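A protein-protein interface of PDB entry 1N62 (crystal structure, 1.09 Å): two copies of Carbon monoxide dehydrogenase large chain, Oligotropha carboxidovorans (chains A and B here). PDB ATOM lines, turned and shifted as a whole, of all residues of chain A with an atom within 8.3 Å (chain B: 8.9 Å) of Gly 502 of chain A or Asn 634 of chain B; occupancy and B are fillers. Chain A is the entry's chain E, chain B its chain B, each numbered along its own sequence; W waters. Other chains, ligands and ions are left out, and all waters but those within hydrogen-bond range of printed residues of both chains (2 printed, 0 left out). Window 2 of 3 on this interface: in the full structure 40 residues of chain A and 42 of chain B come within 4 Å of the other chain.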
ATOM      1  N   LEU A  98      13.434   0.676  37.441  1.00  0.00           N
ATOM      2  CA  LEU A  98      13.202   1.380  36.205  1.00  0.00           C
ATOM      3  C   LEU A  98      14.084   2.583  36.101  1.00  0.00           C
ATOM      4  O   LEU A  98      14.264   3.124  35.046  1.00  0.00           O
ATOM      5  CB  LEU A  98      11.740   1.776  36.095  1.00  0.00           C
ATOM      6  CG  LEU A  98      10.798   0.594  35.880  1.00  0.00           C
ATOM      7  CD1 LEU A  98       9.407   1.129  35.622  1.00  0.00           C
ATOM      8  CD2 LEU A  98      11.272  -0.256  34.751  1.00  0.00           C
ATOM      9  N   ASP A 347      10.241   5.947  35.306  1.00  0.00           N
ATOM     10  CA  ASP A 347      10.465   7.008  34.361  1.00  0.00           C
ATOM     11  C   ASP A 347      10.983   6.291  33.128  1.00  0.00           C
ATOM     12  O   ASP A 347      11.645   5.250  33.217  1.00  0.00           O
ATOM     13  CB  ASP A 347      11.554   7.967  34.809  1.00  0.00           C
ATOM     14  CG  ASP A 347      11.042   9.078  35.644  1.00  0.00           C
ATOM     15  OD1 ASP A 347      10.026   9.701  35.295  1.00  0.00           O
ATOM     16  OD2 ASP A 347      11.668   9.394  36.679  1.00  0.00           O
ATOM     17  N   PRO A 348      10.861   6.922  31.986  1.00  0.00           N
ATOM     18  CA  PRO A 348      11.667   6.497  30.839  1.00  0.00           C
ATOM     19  C   PRO A 348      13.118   6.686  31.220  1.00  0.00           C
ATOM     20  O   PRO A 348      13.463   7.557  32.015  1.00  0.00           O
ATOM     21  CB  PRO A 348      11.228   7.435  29.732  1.00  0.00           C
ATOM     22  CG  PRO A 348      10.001   8.131  30.265  1.00  0.00           C
ATOM     23  CD  PRO A 348      10.122   8.163  31.726  1.00  0.00           C
ATOM     24  N   SER A 349      13.983   5.881  30.672  1.00  0.00           N
ATOM     25  CA  SER A 349      15.321   5.768  31.196  1.00  0.00           C
ATOM     26  C   SER A 349      16.152   7.016  31.073  1.00  0.00           C
ATOM     27  O   SER A 349      17.074   7.212  31.852  1.00  0.00           O
ATOM     28  CB  SER A 349      16.057   4.610  30.550  1.00  0.00           C
ATOM     29  OG  SER A 349      16.438   4.957  29.251  1.00  0.00           O
ATOM     30  N   LYS A 350      15.803   7.886  30.144  1.00  0.00           N
ATOM     31  CA  LYS A 350      16.562   9.087  29.960  1.00  0.00           C
ATOM     32  C   LYS A 350      16.086  10.248  30.786  1.00  0.00           C
ATOM     33  O   LYS A 350      16.560  11.341  30.616  1.00  0.00           O
ATOM     34  CB  LYS A 350      16.606   9.458  28.489  1.00  0.00           C
ATOM     35  CG  LYS A 350      17.288   8.400  27.632  1.00  0.00           C
ATOM     36  CD  LYS A 350      17.060   8.659  26.164  1.00  0.00           C
ATOM     37  CE  LYS A 350      17.822   7.682  25.329  1.00  0.00           C
ATOM     38  NZ  LYS A 350      17.379   7.809  23.925  1.00  0.00           N
ATOM     39  N   SER A 495      10.080   6.706  20.195  1.00  0.00           N
ATOM     40  CA  SER A 495      11.189   5.817  20.477  1.00  0.00           C
ATOM     41  C   SER A 495      12.490   6.581  20.641  1.00  0.00           C
ATOM     42  O   SER A 495      13.402   6.103  21.296  1.00  0.00           O
ATOM     43  CB  SER A 495      11.318   4.758  19.389  1.00  0.00           C
ATOM     44  OG  SER A 495      11.382   5.331  18.092  1.00  0.00           O
ATOM     45  N   LYS A 496      12.599   7.726  19.986  1.00  0.00           N
ATOM     46  CA  LYS A 496      13.835   8.500  20.032  1.00  0.00           C
ATOM     47  C   LYS A 496      14.260   8.728  21.480  1.00  0.00           C
ATOM     48  O   LYS A 496      15.453   8.716  21.791  1.00  0.00           O
ATOM     49  CB  LYS A 496      13.664   9.841  19.300  1.00  0.00           C
ATOM     50  N   ASN A 497      13.301   9.006  22.356  1.00  0.00           N
ATOM     51  CA  ASN A 497      13.677   9.498  23.655  1.00  0.00           C
ATOM     52  C   ASN A 497      12.987   8.781  24.787  1.00  0.00           C
ATOM     53  O   ASN A 497      13.248   9.092  25.916  1.00  0.00           O
ATOM     54  CB  ASN A 497      13.439  10.997  23.743  1.00  0.00           C
ATOM     55  CG  ASN A 497      11.985  11.374  23.570  1.00  0.00           C
ATOM     56  OD1 ASN A 497      11.141  10.596  23.145  1.00  0.00           O
ATOM     57  N   CYS A 498      12.011   7.934  24.491  1.00  0.00           N
ATOM     58  CA  CYS A 498      11.221   7.292  25.516  1.00  0.00           C
ATOM     59  C   CYS A 498      11.428   5.806  25.424  1.00  0.00           C
ATOM     60  O   CYS A 498      11.017   5.176  24.473  1.00  0.00           O
ATOM     61  CB  CYS A 498       9.752   7.615  25.365  1.00  0.00           C
ATOM     62  SG  CYS A 498       9.409   9.326  25.718  1.00  0.00           S
ATOM     63  N   ASP A 499      11.990   5.249  26.477  1.00  0.00           N
ATOM     64  CA  ASP A 499      12.142   3.829  26.593  1.00  0.00           C
ATOM     65  C   ASP A 499      12.081   3.467  28.049  1.00  0.00           C
ATOM     66  O   ASP A 499      12.447   4.237  28.911  1.00  0.00           O
ATOM     67  CB  ASP A 499      13.477   3.396  25.997  1.00  0.00           C
ATOM     68  CG  ASP A 499      14.626   3.901  26.788  1.00  0.00           C
ATOM     69  OD1 ASP A 499      15.091   5.022  26.525  1.00  0.00           O
ATOM     70  OD2 ASP A 499      15.132   3.208  27.683  1.00  0.00           O
ATOM     71  N   ILE A 500      11.588   2.287  28.300  1.00  0.00           N
ATOM     72  CA  ILE A 500      11.613   1.724  29.629  1.00  0.00           C
ATOM     73  C   ILE A 500      12.661   0.660  29.593  1.00  0.00           C
ATOM     74  O   ILE A 500      12.523  -0.368  28.916  1.00  0.00           O
ATOM     75  CB  ILE A 500      10.266   1.109  29.986  1.00  0.00           C
ATOM     76  CG1 ILE A 500       9.185   2.171  30.046  1.00  0.00           C
ATOM     77  CG2 ILE A 500      10.361   0.353  31.280  1.00  0.00           C
ATOM     78  CD1 ILE A 500       9.313   3.166  31.204  1.00  0.00           C
ATOM     79  N   LEU A 501      13.740   0.962  30.295  1.00  0.00           N
ATOM     80  CA  LEU A 501      14.910   0.125  30.330  1.00  0.00           C
ATOM     81  C   LEU A 501      15.187  -0.429  28.944  1.00  0.00           C
ATOM     82  O   LEU A 501      15.588  -1.569  28.779  1.00  0.00           O
ATOM     83  CB  LEU A 501      14.702  -0.996  31.324  1.00  0.00           C
ATOM     84  CG  LEU A 501      14.511  -0.500  32.762  1.00  0.00           C
ATOM     85  CD1 LEU A 501      14.361  -1.667  33.683  1.00  0.00           C
ATOM     86  CD2 LEU A 501      15.653   0.382  33.225  1.00  0.00           C
ATOM     87  N   GLY A 502      15.258   0.475  27.995  1.00  0.00           N
ATOM     88  CA  GLY A 502      15.704   0.109  26.665  1.00  0.00           C
ATOM     89  C   GLY A 502      14.642  -0.390  25.711  1.00  0.00           C
ATOM     90  O   GLY A 502      14.898  -0.540  24.530  1.00  0.00           O
ATOM     91  N   VAL A 503      13.439  -0.626  26.198  1.00  0.00           N
ATOM     92  CA  VAL A 503      12.345  -0.945  25.313  1.00  0.00           C
ATOM     93  C   VAL A 503      11.636   0.336  24.971  1.00  0.00           C
ATOM     94  O   VAL A 503      11.143   1.046  25.836  1.00  0.00           O
ATOM     95  CB  VAL A 503      11.373  -1.912  25.942  1.00  0.00           C
ATOM     96  CG1 VAL A 503      10.262  -2.203  24.986  1.00  0.00           C
ATOM     97  CG2 VAL A 503      12.068  -3.176  26.315  1.00  0.00           C
ATOM     98  N   SER A 504      11.587   0.641  23.686  1.00  0.00           N
ATOM     99  CA  SER A 504      10.940   1.855  23.253  1.00  0.00           C
ATOM    100  C   SER A 504       9.494   1.868  23.649  1.00  0.00           C
ATOM    101  O   SER A 504       8.832   0.862  23.673  1.00  0.00           O
ATOM    102  CB  SER A 504      11.111   2.054  21.742  1.00  0.00           C
ATOM    103  OG  SER A 504      10.483   1.033  20.997  1.00  0.00           O
ATOM    104  N   MET A 505       8.989   3.062  23.936  1.00  0.00           N
ATOM    105  CA  MET A 505       7.673   3.185  24.538  1.00  0.00           C
ATOM    106  C   MET A 505       6.570   3.269  23.498  1.00  0.00           C
ATOM    107  O   MET A 505       5.788   4.199  23.450  1.00  0.00           O
ATOM    108  CB  MET A 505       7.665   4.334  25.515  1.00  0.00           C
ATOM    109  CG  MET A 505       8.544   4.036  26.695  1.00  0.00           C
ATOM    110  SD  MET A 505       8.492   5.260  27.981  1.00  0.00           S
ATOM    111  CE  MET A 505       6.930   4.940  28.697  1.00  0.00           C
ATOM    112  N   PHE A 506       6.500   2.229  22.688  1.00  0.00           N
ATOM    113  CA  PHE A 506       5.403   2.070  21.751  1.00  0.00           C
ATOM    114  C   PHE A 506       4.235   1.413  22.449  1.00  0.00           C
ATOM    115  O   PHE A 506       4.344   1.046  23.601  1.00  0.00           O
ATOM    116  CB  PHE A 506       5.857   1.235  20.559  1.00  0.00           C
ATOM    117  CG  PHE A 506       6.302  -0.125  20.940  1.00  0.00           C
ATOM    118  CD1 PHE A 506       5.398  -1.154  21.094  1.00  0.00           C
ATOM    119  CD2 PHE A 506       7.624  -0.368  21.199  1.00  0.00           C
ATOM    120  CE1 PHE A 506       5.802  -2.365  21.590  1.00  0.00           C
ATOM    121  CE2 PHE A 506       8.033  -1.595  21.662  1.00  0.00           C
ATOM    122  CZ  PHE A 506       7.124  -2.590  21.829  1.00  0.00           C
ATOM    123  N   TYR A 563       3.067  -7.251  22.415  1.00  0.00           N
ATOM    124  CA  TYR A 563       3.910  -6.601  23.377  1.00  0.00           C
ATOM    125  C   TYR A 563       3.548  -5.162  23.458  1.00  0.00           C
ATOM    126  O   TYR A 563       3.435  -4.495  22.453  1.00  0.00           O
ATOM    127  CB  TYR A 563       5.371  -6.775  22.992  1.00  0.00           C
ATOM    128  CG  TYR A 563       6.332  -6.539  24.112  1.00  0.00           C
ATOM    129  CD1 TYR A 563       6.631  -5.264  24.530  1.00  0.00           C
ATOM    130  CD2 TYR A 563       6.932  -7.584  24.781  1.00  0.00           C
ATOM    131  CE1 TYR A 563       7.482  -5.046  25.571  1.00  0.00           C
ATOM    132  CE2 TYR A 563       7.792  -7.380  25.814  1.00  0.00           C
ATOM    133  CZ  TYR A 563       8.060  -6.104  26.225  1.00  0.00           C
ATOM    134  OH  TYR A 563       8.919  -5.894  27.275  1.00  0.00           O
ATOM    135  N   LEU A 565       3.881  -1.595  26.408  1.00  0.00           N
ATOM    136  CA  LEU A 565       4.605  -1.009  27.511  1.00  0.00           C
ATOM    137  C   LEU A 565       3.736  -0.752  28.707  1.00  0.00           C
ATOM    138  O   LEU A 565       4.226  -0.332  29.728  1.00  0.00           O
ATOM    139  CB  LEU A 565       5.304   0.230  27.034  1.00  0.00           C
ATOM    140  CG  LEU A 565       6.663  -0.030  26.371  1.00  0.00           C
ATOM    141  CD1 LEU A 565       7.683  -0.519  27.367  1.00  0.00           C
ATOM    142  CD2 LEU A 565       6.558  -1.004  25.206  1.00  0.00           C
ATOM    143  N   PRO B 515      11.483  -9.599  22.926  1.00  0.00           N
ATOM    144  CA  PRO B 515      12.658  -8.718  22.900  1.00  0.00           C
ATOM    145  C   PRO B 515      13.953  -9.463  23.094  1.00  0.00           C
ATOM    146  O   PRO B 515      14.963  -9.066  22.536  1.00  0.00           O
ATOM    147  CB  PRO B 515      12.398  -7.740  24.047  1.00  0.00           C
ATOM    148  CG  PRO B 515      10.909  -7.678  24.107  1.00  0.00           C
ATOM    149  CD  PRO B 515      10.425  -9.094  23.807  1.00  0.00           C
ATOM    150  N   ILE B 594      16.058  -4.372   9.351  1.00  0.00           N
ATOM    151  CA  ILE B 594      16.652  -3.849  10.561  1.00  0.00           C
ATOM    152  C   ILE B 594      18.168  -3.964  10.495  1.00  0.00           C
ATOM    153  O   ILE B 594      18.887  -3.047  10.869  1.00  0.00           O
ATOM    154  CB  ILE B 594      16.115  -4.565  11.790  1.00  0.00           C
ATOM    155  CG1 ILE B 594      14.618  -4.337  11.906  1.00  0.00           C
ATOM    156  CG2 ILE B 594      16.832  -4.115  13.027  1.00  0.00           C
ATOM    157  CD1 ILE B 594      13.977  -5.222  12.904  1.00  0.00           C
ATOM    158  N   MET B 598      20.946  -1.042  10.854  1.00  0.00           N
ATOM    159  CA  MET B 598      21.942  -1.043  11.914  1.00  0.00           C
ATOM    160  C   MET B 598      23.343  -1.068  11.368  1.00  0.00           C
ATOM    161  O   MET B 598      24.228  -0.406  11.899  1.00  0.00           O
ATOM    162  CB  MET B 598      21.751  -2.239  12.820  1.00  0.00           C
ATOM    163  CG  MET B 598      20.484  -2.177  13.577  1.00  0.00           C
ATOM    164  SD  MET B 598      20.248  -3.532  14.654  1.00  0.00           S
ATOM    165  CE  MET B 598      21.239  -3.032  16.010  1.00  0.00           C
ATOM    166  N   LYS B 626      19.082 -12.635  17.064  1.00  0.00           N
ATOM    167  CA  LYS B 626      18.816 -12.268  18.423  1.00  0.00           C
ATOM    168  C   LYS B 626      19.010 -10.779  18.637  1.00  0.00           C
ATOM    169  O   LYS B 626      18.170 -10.101  19.249  1.00  0.00           O
ATOM    170  CB  LYS B 626      19.733 -13.043  19.353  1.00  0.00           C
ATOM    171  CG  LYS B 626      19.481 -12.736  20.782  1.00  0.00           C
ATOM    172  CD  LYS B 626      20.116 -13.748  21.690  1.00  0.00           C
ATOM    173  CE  LYS B 626      19.839 -13.389  23.141  1.00  0.00           C
ATOM    174  N   GLU B 627      20.087 -10.244  18.092  1.00  0.00           N
ATOM    175  CA  GLU B 627      20.333  -8.827  18.215  1.00  0.00           C
ATOM    176  C   GLU B 627      19.243  -8.036  17.502  1.00  0.00           C
ATOM    177  O   GLU B 627      18.864  -6.958  17.927  1.00  0.00           O
ATOM    178  CB  GLU B 627      21.696  -8.492  17.602  1.00  0.00           C
ATOM    179  CG  GLU B 627      22.857  -9.011  18.404  1.00  0.00           C
ATOM    180  CD  GLU B 627      24.205  -8.887  17.713  1.00  0.00           C
ATOM    181  OE1 GLU B 627      24.315  -9.015  16.479  1.00  0.00           O
ATOM    182  OE2 GLU B 627      25.193  -8.730  18.451  1.00  0.00           O
ATOM    183  N   LEU B 628      18.796  -8.546  16.371  1.00  0.00           N
ATOM    184  CA  LEU B 628      17.778  -7.860  15.597  1.00  0.00           C
ATOM    185  C   LEU B 628      16.451  -7.849  16.311  1.00  0.00           C
ATOM    186  O   LEU B 628      15.722  -6.873  16.237  1.00  0.00           O
ATOM    187  CB  LEU B 628      17.691  -8.485  14.199  1.00  0.00           C
ATOM    188  CG  LEU B 628      18.991  -8.320  13.444  1.00  0.00           C
ATOM    189  CD1 LEU B 628      18.997  -9.223  12.239  1.00  0.00           C
ATOM    190  CD2 LEU B 628      19.219  -6.894  13.053  1.00  0.00           C
ATOM    191  N   ALA B 629      16.135  -8.944  16.987  1.00  0.00           N
ATOM    192  CA  ALA B 629      14.917  -8.988  17.733  1.00  0.00           C
ATOM    193  C   ALA B 629      14.967  -7.922  18.814  1.00  0.00           C
ATOM    194  O   ALA B 629      14.007  -7.172  18.999  1.00  0.00           O
ATOM    195  CB  ALA B 629      14.742 -10.335  18.339  1.00  0.00           C
ATOM    196  N   TRP B 630      16.081  -7.808  19.531  1.00  0.00           N
ATOM    197  CA  TRP B 630      16.152  -6.798  20.545  1.00  0.00           C
ATOM    198  C   TRP B 630      16.045  -5.440  19.890  1.00  0.00           C
ATOM    199  O   TRP B 630      15.335  -4.566  20.370  1.00  0.00           O
ATOM    200  CB  TRP B 630      17.459  -6.910  21.305  1.00  0.00           C
ATOM    201  CG  TRP B 630      17.702  -5.817  22.283  1.00  0.00           C
ATOM    202  CD1 TRP B 630      18.636  -4.863  22.171  1.00  0.00           C
ATOM    203  CD2 TRP B 630      16.873  -5.422  23.368  1.00  0.00           C
ATOM    204  NE1 TRP B 630      18.566  -3.993  23.228  1.00  0.00           N
ATOM    205  CE2 TRP B 630      17.463  -4.299  23.959  1.00  0.00           C
ATOM    206  CE3 TRP B 630      15.691  -5.901  23.921  1.00  0.00           C
ATOM    207  CZ2 TRP B 630      16.949  -3.696  25.091  1.00  0.00           C
ATOM    208  CZ3 TRP B 630      15.222  -5.337  25.066  1.00  0.00           C
ATOM    209  CH2 TRP B 630      15.841  -4.235  25.640  1.00  0.00           C
ATOM    210  N   ALA B 631      16.783  -5.239  18.818  1.00  0.00           N
ATOM    211  CA  ALA B 631      16.736  -3.977  18.146  1.00  0.00           C
ATOM    212  C   ALA B 631      15.318  -3.588  17.752  1.00  0.00           C
ATOM    213  O   ALA B 631      14.974  -2.405  17.736  1.00  0.00           O
ATOM    214  CB  ALA B 631      17.662  -3.965  16.961  1.00  0.00           C
ATOM    215  N   SER B 632      14.510  -4.548  17.350  1.00  0.00           N
ATOM    216  CA  SER B 632      13.194  -4.193  16.895  1.00  0.00           C
ATOM    217  C   SER B 632      12.351  -3.565  17.983  1.00  0.00           C
ATOM    218  O   SER B 632      11.378  -2.876  17.699  1.00  0.00           O
ATOM    219  CB  SER B 632      12.482  -5.429  16.335  1.00  0.00           C
ATOM    220  OG  SER B 632      12.034  -6.247  17.368  1.00  0.00           O
ATOM    221  N   TYR B 633      12.715  -3.833  19.228  1.00  0.00           N
ATOM    222  CA  TYR B 633      12.047  -3.235  20.385  1.00  0.00           C
ATOM    223  C   TYR B 633      12.795  -2.021  20.918  1.00  0.00           C
ATOM    224  O   TYR B 633      12.193  -1.094  21.442  1.00  0.00           O
ATOM    225  CB  TYR B 633      11.906  -4.260  21.501  1.00  0.00           C
ATOM    226  CG  TYR B 633      10.941  -5.349  21.200  1.00  0.00           C
ATOM    227  CD1 TYR B 633      11.335  -6.477  20.549  1.00  0.00           C
ATOM    228  CD2 TYR B 633       9.620  -5.277  21.594  1.00  0.00           C
ATOM    229  CE1 TYR B 633      10.456  -7.471  20.268  1.00  0.00           C
ATOM    230  CE2 TYR B 633       8.741  -6.289  21.344  1.00  0.00           C
ATOM    231  CZ  TYR B 633       9.187  -7.403  20.718  1.00  0.00           C
ATOM    232  OH  TYR B 633       8.325  -8.459  20.577  1.00  0.00           O
ATOM    233  N   ASN B 634      14.109  -2.098  20.851  1.00  0.00           N
ATOM    234  CA  ASN B 634      14.979  -1.159  21.533  1.00  0.00           C
ATOM    235  C   ASN B 634      15.254   0.020  20.642  1.00  0.00           C
ATOM    236  O   ASN B 634      15.419   1.136  21.097  1.00  0.00           O
ATOM    237  CB  ASN B 634      16.266  -1.895  21.907  1.00  0.00           C
ATOM    238  CG  ASN B 634      17.408  -0.974  22.232  1.00  0.00           C
ATOM    239  OD1 ASN B 634      18.365  -0.854  21.456  1.00  0.00           O
ATOM    240  ND2 ASN B 634      17.351  -0.352  23.394  1.00  0.00           N
ATOM    241  N   SER B 635      15.480  -0.255  19.373  1.00  0.00           N
ATOM    242  CA  SER B 635      15.883   0.772  18.437  1.00  0.00           C
ATOM    243  C   SER B 635      15.194   0.581  17.103  1.00  0.00           C
ATOM    244  O   SER B 635      15.839   0.313  16.102  1.00  0.00           O
ATOM    245  CB  SER B 635      17.391   0.705  18.194  1.00  0.00           C
ATOM    246  N   PRO B 636      13.874   0.593  17.090  1.00  0.00           N
ATOM    247  CA  PRO B 636      13.167   0.317  15.840  1.00  0.00           C
ATOM    248  C   PRO B 636      13.581   1.329  14.785  1.00  0.00           C
ATOM    249  O   PRO B 636      13.686   2.486  15.092  1.00  0.00           O
ATOM    250  CB  PRO B 636      11.692   0.494  16.229  1.00  0.00           C
ATOM    251  CG  PRO B 636      11.704   1.228  17.492  1.00  0.00           C
ATOM    252  CD  PRO B 636      12.965   0.900  18.214  1.00  0.00           C
ATOM    253  N   PRO B 637      14.006   0.878  13.618  1.00  0.00           N
ATOM    254  CA  PRO B 637      14.309   1.818  12.546  1.00  0.00           C
ATOM    255  C   PRO B 637      13.115   2.709  12.260  1.00  0.00           C
ATOM    256  O   PRO B 637      11.982   2.289  12.446  1.00  0.00           O
ATOM    257  CB  PRO B 637      14.646   0.921  11.366  1.00  0.00           C
ATOM    258  CG  PRO B 637      15.044  -0.377  11.985  1.00  0.00           C
ATOM    259  CD  PRO B 637      14.226  -0.519  13.208  1.00  0.00           C
ATOM    260  N   GLU B 641       7.639  -0.510  12.036  1.00  0.00           N
ATOM    261  CA  GLU B 641       7.004  -0.629  13.326  1.00  0.00           C
ATOM    262  C   GLU B 641       7.949  -1.333  14.249  1.00  0.00           C
ATOM    263  O   GLU B 641       8.693  -2.203  13.842  1.00  0.00           O
ATOM    264  CB  GLU B 641       5.724  -1.452  13.214  1.00  0.00           C
ATOM    265  CG  GLU B 641       4.687  -0.801  12.325  1.00  0.00           C
ATOM    266  CD  GLU B 641       3.384  -1.538  12.238  1.00  0.00           C
ATOM    267  OE1 GLU B 641       3.078  -2.331  13.141  1.00  0.00           O
ATOM    268  OE2 GLU B 641       2.613  -1.231  11.301  1.00  0.00           O
ATOM    269  N   PRO B 642       7.846  -1.041  15.528  1.00  0.00           N
ATOM    270  CA  PRO B 642       8.555  -1.848  16.508  1.00  0.00           C
ATOM    271  C   PRO B 642       8.063  -3.267  16.495  1.00  0.00           C
ATOM    272  O   PRO B 642       7.014  -3.584  15.953  1.00  0.00           O
ATOM    273  CB  PRO B 642       8.193  -1.181  17.844  1.00  0.00           C
ATOM    274  CG  PRO B 642       7.799   0.208  17.489  1.00  0.00           C
ATOM    275  CD  PRO B 642       7.145   0.091  16.145  1.00  0.00           C
ATOM    276  N   GLY B 643       8.860  -4.089  17.136  1.00  0.00           N
ATOM    277  CA  GLY B 643       8.578  -5.488  17.294  1.00  0.00           C
ATOM    278  C   GLY B 643       8.970  -6.301  16.069  1.00  0.00           C
ATOM    279  O   GLY B 643       9.455  -5.807  15.073  1.00  0.00           O
HETATM  280  O   HOH W   1      13.865   4.080  17.447  1.00  0.00           O
HETATM  281  O   HOH W   2      15.575   2.533  23.580  1.00  0.00           O
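OG of Ser 504 of chain A is in hydrogen-bond range of O of Tyr 633 of chain B (2.8 Å). The side-chain amide nitrogen of Asn 634 of chain B lies within hydrogen-bond range of the backbone carbonyl oxygen of Gly 502 of chain A (2.7 Å).
The backbone carbonyl oxygen of Pro 515 of chain B lies close to the backbone NH of Trp 630 of chain B. The side-chain carboxylate of Asp 499 of chain A lies within hydrogen-bond range of the backbone NH of Gly 502 of chain A.
O of Gly 502 of chain A touches CZ2 of Trp 630 of chain B (3.8 Å). CH2 of Trp 630 of chain B touches CG2 of Val 503 of chain A (3.98 Å). O of Tyr 633 of chain B touches C of Val 503 of chain A, at 3.8 Å. Pro 636 of chain B touches Ser 504 of chain A. CZ of Phe 506 of chain A touches CD2 of Tyr 633 of chain B, at 3.7 Å. CB of Pro 642 of chain B touches CD2 of Phe 506 of chain A, at 3.5 Å. Pro 515 of chain B touches Tyr 563 of chain A. Tyr 563 of chain A touches Tyr 633 of chain B (CG to CE2, 3.7 Å).
Gly 502 of chain A touches just these residues of chain B: Trp 630 and Asn 634. Of the printed residues of chain B, Val 503 of chain A touches Trp 630 and Tyr 633. Printed residues of chain A within 4 Å of Tyr 633 of chain B: Val 503, Ser 504, Phe 506 and Tyr 563. Printed residues of chain A within 4 Å of Asn 634 of chain B: Gly 502 (2.7 Å). Of the printed residues of chain A, Pro 636 of chain B touches Ser 504 (3.7 Å). Printed residues of chain A within 4 Å of Pro 642 of chain B: Phe 506. The nearest printed residue of chain A that does not touch Asn 634 of chain B is Ser 504 of chain A (4.4 Å). The nearest printed residue of chain A that does not touch Trp 630 of chain B is Leu 501 of chain A (4.1 Å).
Printed residues of chain A that touch a printed residue of chain B: Gly 502, Val 503, Ser 504, Phe 506 and Tyr 563. Hydrophobic or aromatic side chains of chain A within 4 Å of the printed part of chain B: Val 503, Phe 506 and Tyr 563. Among the printed residues, 10 pairs touch across the chains. Among the printed residues, no Asp or Glu carboxylate lies within 4 Å of a Lys or Arg side-chain nitrogen of the other chain.
No position is printed for both chains.
Water W1 bridges the backbone carbonyl oxygen of Pro 636 of chain B (2.8 Å) and the side-chain hydroxyl of Ser 495 of chain A (2.9 Å). Water W2 lies within hydrogen-bond range of O of Asn 634 of chain B (2.9 Å) and O of Gly 502 of chain A (3.3 Å).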
